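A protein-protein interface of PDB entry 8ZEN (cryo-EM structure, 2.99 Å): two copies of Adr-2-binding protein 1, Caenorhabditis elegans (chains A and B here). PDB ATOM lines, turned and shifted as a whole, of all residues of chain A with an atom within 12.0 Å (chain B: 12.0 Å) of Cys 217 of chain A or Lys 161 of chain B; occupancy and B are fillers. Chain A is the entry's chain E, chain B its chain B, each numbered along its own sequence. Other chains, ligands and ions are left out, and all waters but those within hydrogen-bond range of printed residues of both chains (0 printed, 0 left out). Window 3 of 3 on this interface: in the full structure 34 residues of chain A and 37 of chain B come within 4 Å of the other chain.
Hydrophobic or aromatic side chains of chain A within 4 Å of the printed part of chain B: Ile 207 and Ile 214.
Printed residues of chain B that touch a printed residue of chain A: Val 160, Lys 161, Val 164, Leu 167, Val 187 and Arg 190.
Hydrophobic or aromatic side chains of chain B within 4 Å of the printed part of chain A: Val 160, Val 164, Leu 167 and Val 187.
Along chain B the printed residues that touch a printed residue of chain A span positions 160 to 190.
Among the printed residues, 8 pairs touch across the chains.
Among the printed residues, no Asp or Glu carboxylate lies within 4 Å of a Lys or Arg side-chain nitrogen of the other chain.
Among the printed residues, merely in contact across the chains: Ile 214 of chain A with Val 160 of chain B, Val 215 of chain A with Val 160 of chain B, Ile 214 of chain A with Arg 190 of chain B, Cys 217 of chain A with Val 160 of chain B, Val 215 of chain A with Val 164 of chain B, Ile 207 of chain A with Val 187 of chain B, Ile 207 of chain A with Leu 167 of chain B and Cys 217 of chain A with Lys 161 of chain B.
The backbone carbonyl oxygen (O) of Met 158 of chain B sits at hydrogen-bond distance from the guanidinium group (NH2) of Arg 190 of chain B, 2.9 Å away.
Printed residues of chain B within 4 Å of Ile 207 of chain A: Leu 167 (3.8 Å) and Val 187 (3.7 Å).
No residue of chain B comes within 4 Å of Asn 216 of chain A.
Cys 217 of chain A touches just these residues of chain B: Val 160 (3.6 Å) and Lys 161 (3.9 Å).
Asp 159 of chain B touches none of the printed residues of chain A.
Val 160 of chain B touches just these residues of chain A: Ile 214, Val 215 and Cys 217.
Lys 161 of chain B touches just one residue of chain A: Cys 217.
No residue of chain A comes within 4 Å of Ile 163 of chain B.
Val 164 of chain B touches one residue of chain A.
Printed residues of chain A within 4 Å of Arg 190 of chain B: Ile 214.
The nearest residue of chain A that does not touch Lys 161 of chain B is Val 215 of chain A (5.9 Å).
No position is printed for both chains.
Of the 8 pairs that touch across the chains among the printed residues, none has its exchanged pair printed and touching as well.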
ATOM      1  N   ILE A 207       8.925   5.906  18.833  1.00  0.00           N
ATOM      2  CA  ILE A 207       8.527   5.954  20.238  1.00  0.00           C
ATOM      3  C   ILE A 207       9.754   5.952  21.141  1.00  0.00           C
ATOM      4  O   ILE A 207       9.865   6.763  22.068  1.00  0.00           O
ATOM      5  CB  ILE A 207       7.575   4.790  20.566  1.00  0.00           C
ATOM      6  CG1 ILE A 207       6.205   5.037  19.932  1.00  0.00           C
ATOM      7  CG2 ILE A 207       7.451   4.613  22.069  1.00  0.00           C
ATOM      8  CD1 ILE A 207       5.102   4.163  20.483  1.00  0.00           C
ATOM      9  N   GLU A 208      10.704   5.051  20.878  1.00  0.00           N
ATOM     10  CA  GLU A 208      11.897   4.976  21.717  1.00  0.00           C
ATOM     11  C   GLU A 208      12.828   6.170  21.547  1.00  0.00           C
ATOM     12  O   GLU A 208      13.674   6.393  22.419  1.00  0.00           O
ATOM     13  CB  GLU A 208      12.688   3.691  21.452  1.00  0.00           C
ATOM     14  CG  GLU A 208      11.852   2.450  21.234  1.00  0.00           C
ATOM     15  CD  GLU A 208      11.843   1.533  22.439  1.00  0.00           C
ATOM     16  OE1 GLU A 208      11.746   0.304  22.249  1.00  0.00           O
ATOM     17  OE2 GLU A 208      11.937   2.042  23.576  1.00  0.00           O
ATOM     18  N   LYS A 209      12.710   6.931  20.461  1.00  0.00           N
ATOM     19  CA  LYS A 209      13.596   8.065  20.235  1.00  0.00           C
ATOM     20  C   LYS A 209      13.000   9.371  20.740  1.00  0.00           C
ATOM     21  O   LYS A 209      13.708  10.174  21.355  1.00  0.00           O
ATOM     22  CB  LYS A 209      13.960   8.134  18.730  1.00  0.00           C
ATOM     23  CG  LYS A 209      14.840   9.305  18.199  1.00  0.00           C
ATOM     24  CD  LYS A 209      14.261  10.719  18.231  1.00  0.00           C
ATOM     25  CE  LYS A 209      12.824  10.758  17.741  1.00  0.00           C
ATOM     26  NZ  LYS A 209      12.368  12.152  17.482  1.00  0.00           N
ATOM     27  N   ALA A 211      10.278   9.832  22.926  1.00  0.00           N
ATOM     28  CA  ALA A 211       9.831   9.799  24.320  1.00  0.00           C
ATOM     29  C   ALA A 211      10.456   8.620  25.060  1.00  0.00           C
ATOM     30  O   ALA A 211       9.813   7.592  25.274  1.00  0.00           O
ATOM     31  CB  ALA A 211       8.311   9.739  24.390  1.00  0.00           C
ATOM     32  N   PRO A 212      11.716   8.744  25.478  1.00  0.00           N
ATOM     33  CA  PRO A 212      12.366   7.607  26.145  1.00  0.00           C
ATOM     34  C   PRO A 212      12.068   7.516  27.631  1.00  0.00           C
ATOM     35  O   PRO A 212      12.205   6.436  28.219  1.00  0.00           O
ATOM     36  CB  PRO A 212      13.851   7.864  25.858  1.00  0.00           C
ATOM     37  CG  PRO A 212      13.952   9.386  25.626  1.00  0.00           C
ATOM     38  CD  PRO A 212      12.547   9.954  25.575  1.00  0.00           C
ATOM     39  N   SER A 213      11.658   8.620  28.262  1.00  0.00           N
ATOM     40  CA  SER A 213      11.305   8.570  29.675  1.00  0.00           C
ATOM     41  C   SER A 213      10.024   7.779  29.903  1.00  0.00           C
ATOM     42  O   SER A 213       9.787   7.287  31.012  1.00  0.00           O
ATOM     43  CB  SER A 213      11.157   9.986  30.231  1.00  0.00           C
ATOM     44  OG  SER A 213      12.282  10.781  29.900  1.00  0.00           O
ATOM     45  N   ILE A 214       9.193   7.644  28.867  1.00  0.00           N
ATOM     46  CA  ILE A 214       7.900   6.979  29.014  1.00  0.00           C
ATOM     47  C   ILE A 214       7.966   5.488  28.731  1.00  0.00           C
ATOM     48  O   ILE A 214       7.219   4.720  29.349  1.00  0.00           O
ATOM     49  CB  ILE A 214       6.873   7.685  28.107  1.00  0.00           C
ATOM     50  CG1 ILE A 214       6.215   8.841  28.861  1.00  0.00           C
ATOM     51  CG2 ILE A 214       5.815   6.719  27.589  1.00  0.00           C
ATOM     52  CD1 ILE A 214       5.226   8.399  29.911  1.00  0.00           C
ATOM     53  N   VAL A 215       8.861   5.046  27.849  1.00  0.00           N
ATOM     54  CA  VAL A 215       8.876   3.650  27.423  1.00  0.00           C
ATOM     55  C   VAL A 215       9.911   2.843  28.199  1.00  0.00           C
ATOM     56  O   VAL A 215       9.594   1.781  28.748  1.00  0.00           O
ATOM     57  CB  VAL A 215       9.113   3.543  25.904  1.00  0.00           C
ATOM     58  CG1 VAL A 215      10.300   4.395  25.474  1.00  0.00           C
ATOM     59  CG2 VAL A 215       9.321   2.091  25.504  1.00  0.00           C
ATOM     60  N   ASN A 216      11.149   3.333  28.263  1.00  0.00           N
ATOM     61  CA  ASN A 216      12.236   2.594  28.907  1.00  0.00           C
ATOM     62  C   ASN A 216      12.194   2.783  30.425  1.00  0.00           C
ATOM     63  O   ASN A 216      12.856   3.643  31.005  1.00  0.00           O
ATOM     64  CB  ASN A 216      13.581   3.011  28.326  1.00  0.00           C
ATOM     65  CG  ASN A 216      13.476   3.484  26.891  1.00  0.00           C
ATOM     66  OD1 ASN A 216      13.631   4.668  26.601  1.00  0.00           O
ATOM     67  ND2 ASN A 216      13.207   2.553  25.982  1.00  0.00           N
ATOM     68  N   CYS A 217      11.386   1.944  31.066  1.00  0.00           N
ATOM     69  CA  CYS A 217      11.241   1.962  32.514  1.00  0.00           C
ATOM     70  C   CYS A 217      12.319   1.117  33.184  1.00  0.00           C
ATOM     71  O   CYS A 217      12.758   0.104  32.639  1.00  0.00           O
ATOM     72  CB  CYS A 217       9.855   1.459  32.918  1.00  0.00           C
ATOM     73  SG  CYS A 217       9.443  -0.178  32.267  1.00  0.00           S
ATOM     74  OXT CYS A 217      12.772   1.421  34.287  1.00  0.00           O
ATOM     75  N   GLN B 157      -5.937   1.826  31.610  1.00  0.00           N
ATOM     76  CA  GLN B 157      -4.502   2.032  31.693  1.00  0.00           C
ATOM     77  C   GLN B 157      -3.763   0.703  31.800  1.00  0.00           C
ATOM     78  O   GLN B 157      -4.284  -0.294  32.305  1.00  0.00           O
ATOM     79  CB  GLN B 157      -4.158   2.914  32.890  1.00  0.00           C
ATOM     80  CG  GLN B 157      -4.519   4.371  32.710  1.00  0.00           C
ATOM     81  CD  GLN B 157      -5.016   4.995  33.992  1.00  0.00           C
ATOM     82  OE1 GLN B 157      -4.324   4.980  35.009  1.00  0.00           O
ATOM     83  NE2 GLN B 157      -6.221   5.550  33.953  1.00  0.00           N
ATOM     84  N   MET B 158      -2.528   0.704  31.305  1.00  0.00           N
ATOM     85  CA  MET B 158      -1.658  -0.458  31.387  1.00  0.00           C
ATOM     86  C   MET B 158      -0.248   0.002  31.731  1.00  0.00           C
ATOM     87  O   MET B 158       0.155   1.118  31.394  1.00  0.00           O
ATOM     88  CB  MET B 158      -1.678  -1.253  30.079  1.00  0.00           C
ATOM     89  CG  MET B 158      -1.733  -0.389  28.841  1.00  0.00           C
ATOM     90  SD  MET B 158      -0.890  -1.100  27.417  1.00  0.00           S
ATOM     91  CE  MET B 158      -2.064  -2.361  26.931  1.00  0.00           C
ATOM     92  N   ASP B 159       0.494  -0.869  32.408  1.00  0.00           N
ATOM     93  CA  ASP B 159       1.789  -0.502  32.956  1.00  0.00           C
ATOM     94  C   ASP B 159       2.841  -0.392  31.854  1.00  0.00           C
ATOM     95  O   ASP B 159       2.670  -0.889  30.737  1.00  0.00           O
ATOM     96  CB  ASP B 159       2.232  -1.520  34.008  1.00  0.00           C
ATOM     97  CG  ASP B 159       3.196  -0.931  35.021  1.00  0.00           C
ATOM     98  OD1 ASP B 159       3.556   0.257  34.881  1.00  0.00           O
ATOM     99  OD2 ASP B 159       3.589  -1.658  35.959  1.00  0.00           O
ATOM    100  N   VAL B 160       3.942   0.286  32.189  1.00  0.00           N
ATOM    101  CA  VAL B 160       5.022   0.488  31.226  1.00  0.00           C
ATOM    102  C   VAL B 160       5.669  -0.839  30.858  1.00  0.00           C
ATOM    103  O   VAL B 160       5.973  -1.094  29.686  1.00  0.00           O
ATOM    104  CB  VAL B 160       6.053   1.483  31.783  1.00  0.00           C
ATOM    105  CG1 VAL B 160       6.981   1.936  30.679  1.00  0.00           C
ATOM    106  CG2 VAL B 160       5.355   2.671  32.422  1.00  0.00           C
ATOM    107  N   LYS B 161       5.904  -1.700  31.850  1.00  0.00           N
ATOM    108  CA  LYS B 161       6.424  -3.031  31.561  1.00  0.00           C
ATOM    109  C   LYS B 161       5.489  -3.817  30.656  1.00  0.00           C
ATOM    110  O   LYS B 161       5.953  -4.659  29.879  1.00  0.00           O
ATOM    111  CB  LYS B 161       6.656  -3.799  32.865  1.00  0.00           C
ATOM    112  CG  LYS B 161       5.392  -4.004  33.701  1.00  0.00           C
ATOM    113  CD  LYS B 161       5.622  -4.931  34.888  1.00  0.00           C
ATOM    114  CE  LYS B 161       6.633  -4.359  35.862  1.00  0.00           C
ATOM    115  NZ  LYS B 161       6.766  -5.225  37.065  1.00  0.00           N
ATOM    116  N   GLU B 162       4.183  -3.565  30.753  1.00  0.00           N
ATOM    117  CA  GLU B 162       3.202  -4.160  29.855  1.00  0.00           C
ATOM    118  C   GLU B 162       3.373  -3.638  28.432  1.00  0.00           C
ATOM    119  O   GLU B 162       3.386  -4.428  27.480  1.00  0.00           O
ATOM    120  CB  GLU B 162       1.799  -3.884  30.426  1.00  0.00           C
ATOM    121  CG  GLU B 162       0.600  -3.759  29.483  1.00  0.00           C
ATOM    122  CD  GLU B 162       0.627  -4.673  28.295  1.00  0.00           C
ATOM    123  OE1 GLU B 162       0.632  -4.130  27.171  1.00  0.00           O
ATOM    124  OE2 GLU B 162       0.656  -5.909  28.470  1.00  0.00           O
ATOM    125  N   ILE B 163       3.557  -2.326  28.273  1.00  0.00           N
ATOM    126  CA  ILE B 163       3.590  -1.726  26.939  1.00  0.00           C
ATOM    127  C   ILE B 163       4.744  -2.293  26.122  1.00  0.00           C
ATOM    128  O   ILE B 163       4.595  -2.601  24.934  1.00  0.00           O
ATOM    129  CB  ILE B 163       3.677  -0.193  27.044  1.00  0.00           C
ATOM    130  CG1 ILE B 163       2.321   0.399  27.430  1.00  0.00           C
ATOM    131  CG2 ILE B 163       4.180   0.405  25.741  1.00  0.00           C
ATOM    132  CD1 ILE B 163       2.213   1.884  27.181  1.00  0.00           C
ATOM    133  N   VAL B 164       5.910  -2.450  26.753  1.00  0.00           N
ATOM    134  CA  VAL B 164       7.114  -2.853  26.030  1.00  0.00           C
ATOM    135  C   VAL B 164       6.923  -4.193  25.334  1.00  0.00           C
ATOM    136  O   VAL B 164       7.306  -4.354  24.167  1.00  0.00           O
ATOM    137  CB  VAL B 164       8.316  -2.885  26.995  1.00  0.00           C
ATOM    138  CG1 VAL B 164       9.530  -3.492  26.314  1.00  0.00           C
ATOM    139  CG2 VAL B 164       8.628  -1.485  27.503  1.00  0.00           C
ATOM    140  N   GLU B 165       6.332  -5.170  26.022  1.00  0.00           N
ATOM    141  CA  GLU B 165       6.127  -6.482  25.417  1.00  0.00           C
ATOM    142  C   GLU B 165       5.164  -6.406  24.240  1.00  0.00           C
ATOM    143  O   GLU B 165       5.478  -6.874  23.141  1.00  0.00           O
ATOM    144  CB  GLU B 165       5.614  -7.471  26.465  1.00  0.00           C
ATOM    145  CG  GLU B 165       6.007  -7.120  27.890  1.00  0.00           C
ATOM    146  CD  GLU B 165       5.985  -8.319  28.815  1.00  0.00           C
ATOM    147  OE1 GLU B 165       6.016  -8.125  30.048  1.00  0.00           O
ATOM    148  OE2 GLU B 165       5.931  -9.459  28.309  1.00  0.00           O
ATOM    149  N   LYS B 166       3.993  -5.802  24.449  1.00  0.00           N
ATOM    150  CA  LYS B 166       2.983  -5.760  23.397  1.00  0.00           C
ATOM    151  C   LYS B 166       3.392  -4.845  22.251  1.00  0.00           C
ATOM    152  O   LYS B 166       2.921  -5.024  21.123  1.00  0.00           O
ATOM    153  CB  LYS B 166       1.638  -5.350  23.992  1.00  0.00           C
ATOM    154  CG  LYS B 166       1.104  -6.388  24.976  1.00  0.00           C
ATOM    155  CD  LYS B 166      -0.393  -6.279  25.272  1.00  0.00           C
ATOM    156  CE  LYS B 166      -1.273  -6.532  24.071  1.00  0.00           C
ATOM    157  NZ  LYS B 166      -1.317  -5.368  23.159  1.00  0.00           N
ATOM    158  N   LEU B 167       4.259  -3.868  22.509  1.00  0.00           N
ATOM    159  CA  LEU B 167       4.836  -3.080  21.423  1.00  0.00           C
ATOM    160  C   LEU B 167       5.942  -3.836  20.693  1.00  0.00           C
ATOM    161  O   LEU B 167       6.459  -3.342  19.687  1.00  0.00           O
ATOM    162  CB  LEU B 167       5.353  -1.748  21.979  1.00  0.00           C
ATOM    163  CG  LEU B 167       5.413  -0.474  21.128  1.00  0.00           C
ATOM    164  CD1 LEU B 167       5.300   0.738  22.031  1.00  0.00           C
ATOM    165  CD2 LEU B 167       6.697  -0.383  20.334  1.00  0.00           C
ATOM    166  N   LYS B 168       6.294  -5.036  21.165  1.00  0.00           N
ATOM    167  CA  LYS B 168       7.351  -5.843  20.570  1.00  0.00           C
ATOM    168  C   LYS B 168       6.870  -7.090  19.840  1.00  0.00           C
ATOM    169  O   LYS B 168       7.640  -7.638  19.043  1.00  0.00           O
ATOM    170  CB  LYS B 168       8.365  -6.268  21.649  1.00  0.00           C
ATOM    171  CG  LYS B 168       9.798  -6.620  21.183  1.00  0.00           C
ATOM    172  CD  LYS B 168      10.533  -5.678  20.202  1.00  0.00           C
ATOM    173  CE  LYS B 168      10.156  -4.203  20.257  1.00  0.00           C
ATOM    174  NZ  LYS B 168      11.060  -3.406  19.386  1.00  0.00           N
ATOM    175  N   LYS B 169       5.651  -7.561  20.086  1.00  0.00           N
ATOM    176  CA  LYS B 169       5.187  -8.810  19.496  1.00  0.00           C
ATOM    177  C   LYS B 169       5.134  -8.718  17.973  1.00  0.00           C
ATOM    178  O   LYS B 169       4.851  -7.663  17.401  1.00  0.00           O
ATOM    179  CB  LYS B 169       3.812  -9.183  20.048  1.00  0.00           C
ATOM    180  CG  LYS B 169       3.724  -9.138  21.566  1.00  0.00           C
ATOM    181  CD  LYS B 169       4.840  -9.951  22.206  1.00  0.00           C
ATOM    182  CE  LYS B 169       4.777  -9.894  23.724  1.00  0.00           C
ATOM    183  NZ  LYS B 169       5.870 -10.686  24.353  1.00  0.00           N
ATOM    184  N   GLY B 179      -3.479  -4.891  19.283  1.00  0.00           N
ATOM    185  CA  GLY B 179      -2.595  -4.769  20.428  1.00  0.00           C
ATOM    186  C   GLY B 179      -1.518  -3.715  20.250  1.00  0.00           C
ATOM    187  O   GLY B 179      -1.262  -2.915  21.155  1.00  0.00           O
ATOM    188  N   ALA B 182      -3.064  -0.297  20.415  1.00  0.00           N
ATOM    189  CA  ALA B 182      -3.377   0.051  21.798  1.00  0.00           C
ATOM    190  C   ALA B 182      -2.125   0.472  22.554  1.00  0.00           C
ATOM    191  O   ALA B 182      -2.147   1.439  23.326  1.00  0.00           O
ATOM    192  CB  ALA B 182      -4.056  -1.126  22.494  1.00  0.00           C
ATOM    193  N   ALA B 183      -1.019  -0.245  22.344  1.00  0.00           N
ATOM    194  CA  ALA B 183       0.235   0.144  22.981  1.00  0.00           C
ATOM    195  C   ALA B 183       0.664   1.534  22.534  1.00  0.00           C
ATOM    196  O   ALA B 183       1.091   2.356  23.354  1.00  0.00           O
ATOM    197  CB  ALA B 183       1.323  -0.882  22.667  1.00  0.00           C
ATOM    198  N   ASN B 186      -1.582   4.183  24.285  1.00  0.00           N
ATOM    199  CA  ASN B 186      -1.270   4.442  25.688  1.00  0.00           C
ATOM    200  C   ASN B 186       0.123   5.029  25.871  1.00  0.00           C
ATOM    201  O   ASN B 186       0.382   5.687  26.884  1.00  0.00           O
ATOM    202  CB  ASN B 186      -1.454   3.174  26.516  1.00  0.00           C
ATOM    203  CG  ASN B 186      -2.797   2.529  26.273  1.00  0.00           C
ATOM    204  OD1 ASN B 186      -3.419   2.745  25.237  1.00  0.00           O
ATOM    205  ND2 ASN B 186      -3.272   1.767  27.243  1.00  0.00           N
ATOM    206  N   VAL B 187       1.031   4.817  24.918  1.00  0.00           N
ATOM    207  CA  VAL B 187       2.272   5.587  24.915  1.00  0.00           C
ATOM    208  C   VAL B 187       1.971   7.056  24.649  1.00  0.00           C
ATOM    209  O   VAL B 187       2.497   7.952  25.319  1.00  0.00           O
ATOM    210  CB  VAL B 187       3.263   5.019  23.884  1.00  0.00           C
ATOM    211  CG1 VAL B 187       4.385   6.006  23.634  1.00  0.00           C
ATOM    212  CG2 VAL B 187       3.828   3.707  24.374  1.00  0.00           C
ATOM    213  N   ARG B 190       0.168   8.931  27.776  1.00  0.00           N
ATOM    214  CA  ARG B 190       1.024   9.328  28.883  1.00  0.00           C
ATOM    215  C   ARG B 190       2.096  10.331  28.482  1.00  0.00           C
ATOM    216  O   ARG B 190       2.873  10.761  29.340  1.00  0.00           O
ATOM    217  CB  ARG B 190       1.676   8.093  29.508  1.00  0.00           C
ATOM    218  CG  ARG B 190       0.732   7.289  30.382  1.00  0.00           C
ATOM    219  CD  ARG B 190       1.486   6.492  31.430  1.00  0.00           C
ATOM    220  NE  ARG B 190       1.406   5.056  31.194  1.00  0.00           N
ATOM    221  CZ  ARG B 190       2.228   4.378  30.405  1.00  0.00           C
ATOM    222  NH1 ARG B 190       3.196   4.980  29.736  1.00  0.00           N
ATOM    223  NH2 ARG B 190       2.073   3.063  30.284  1.00  0.00           N
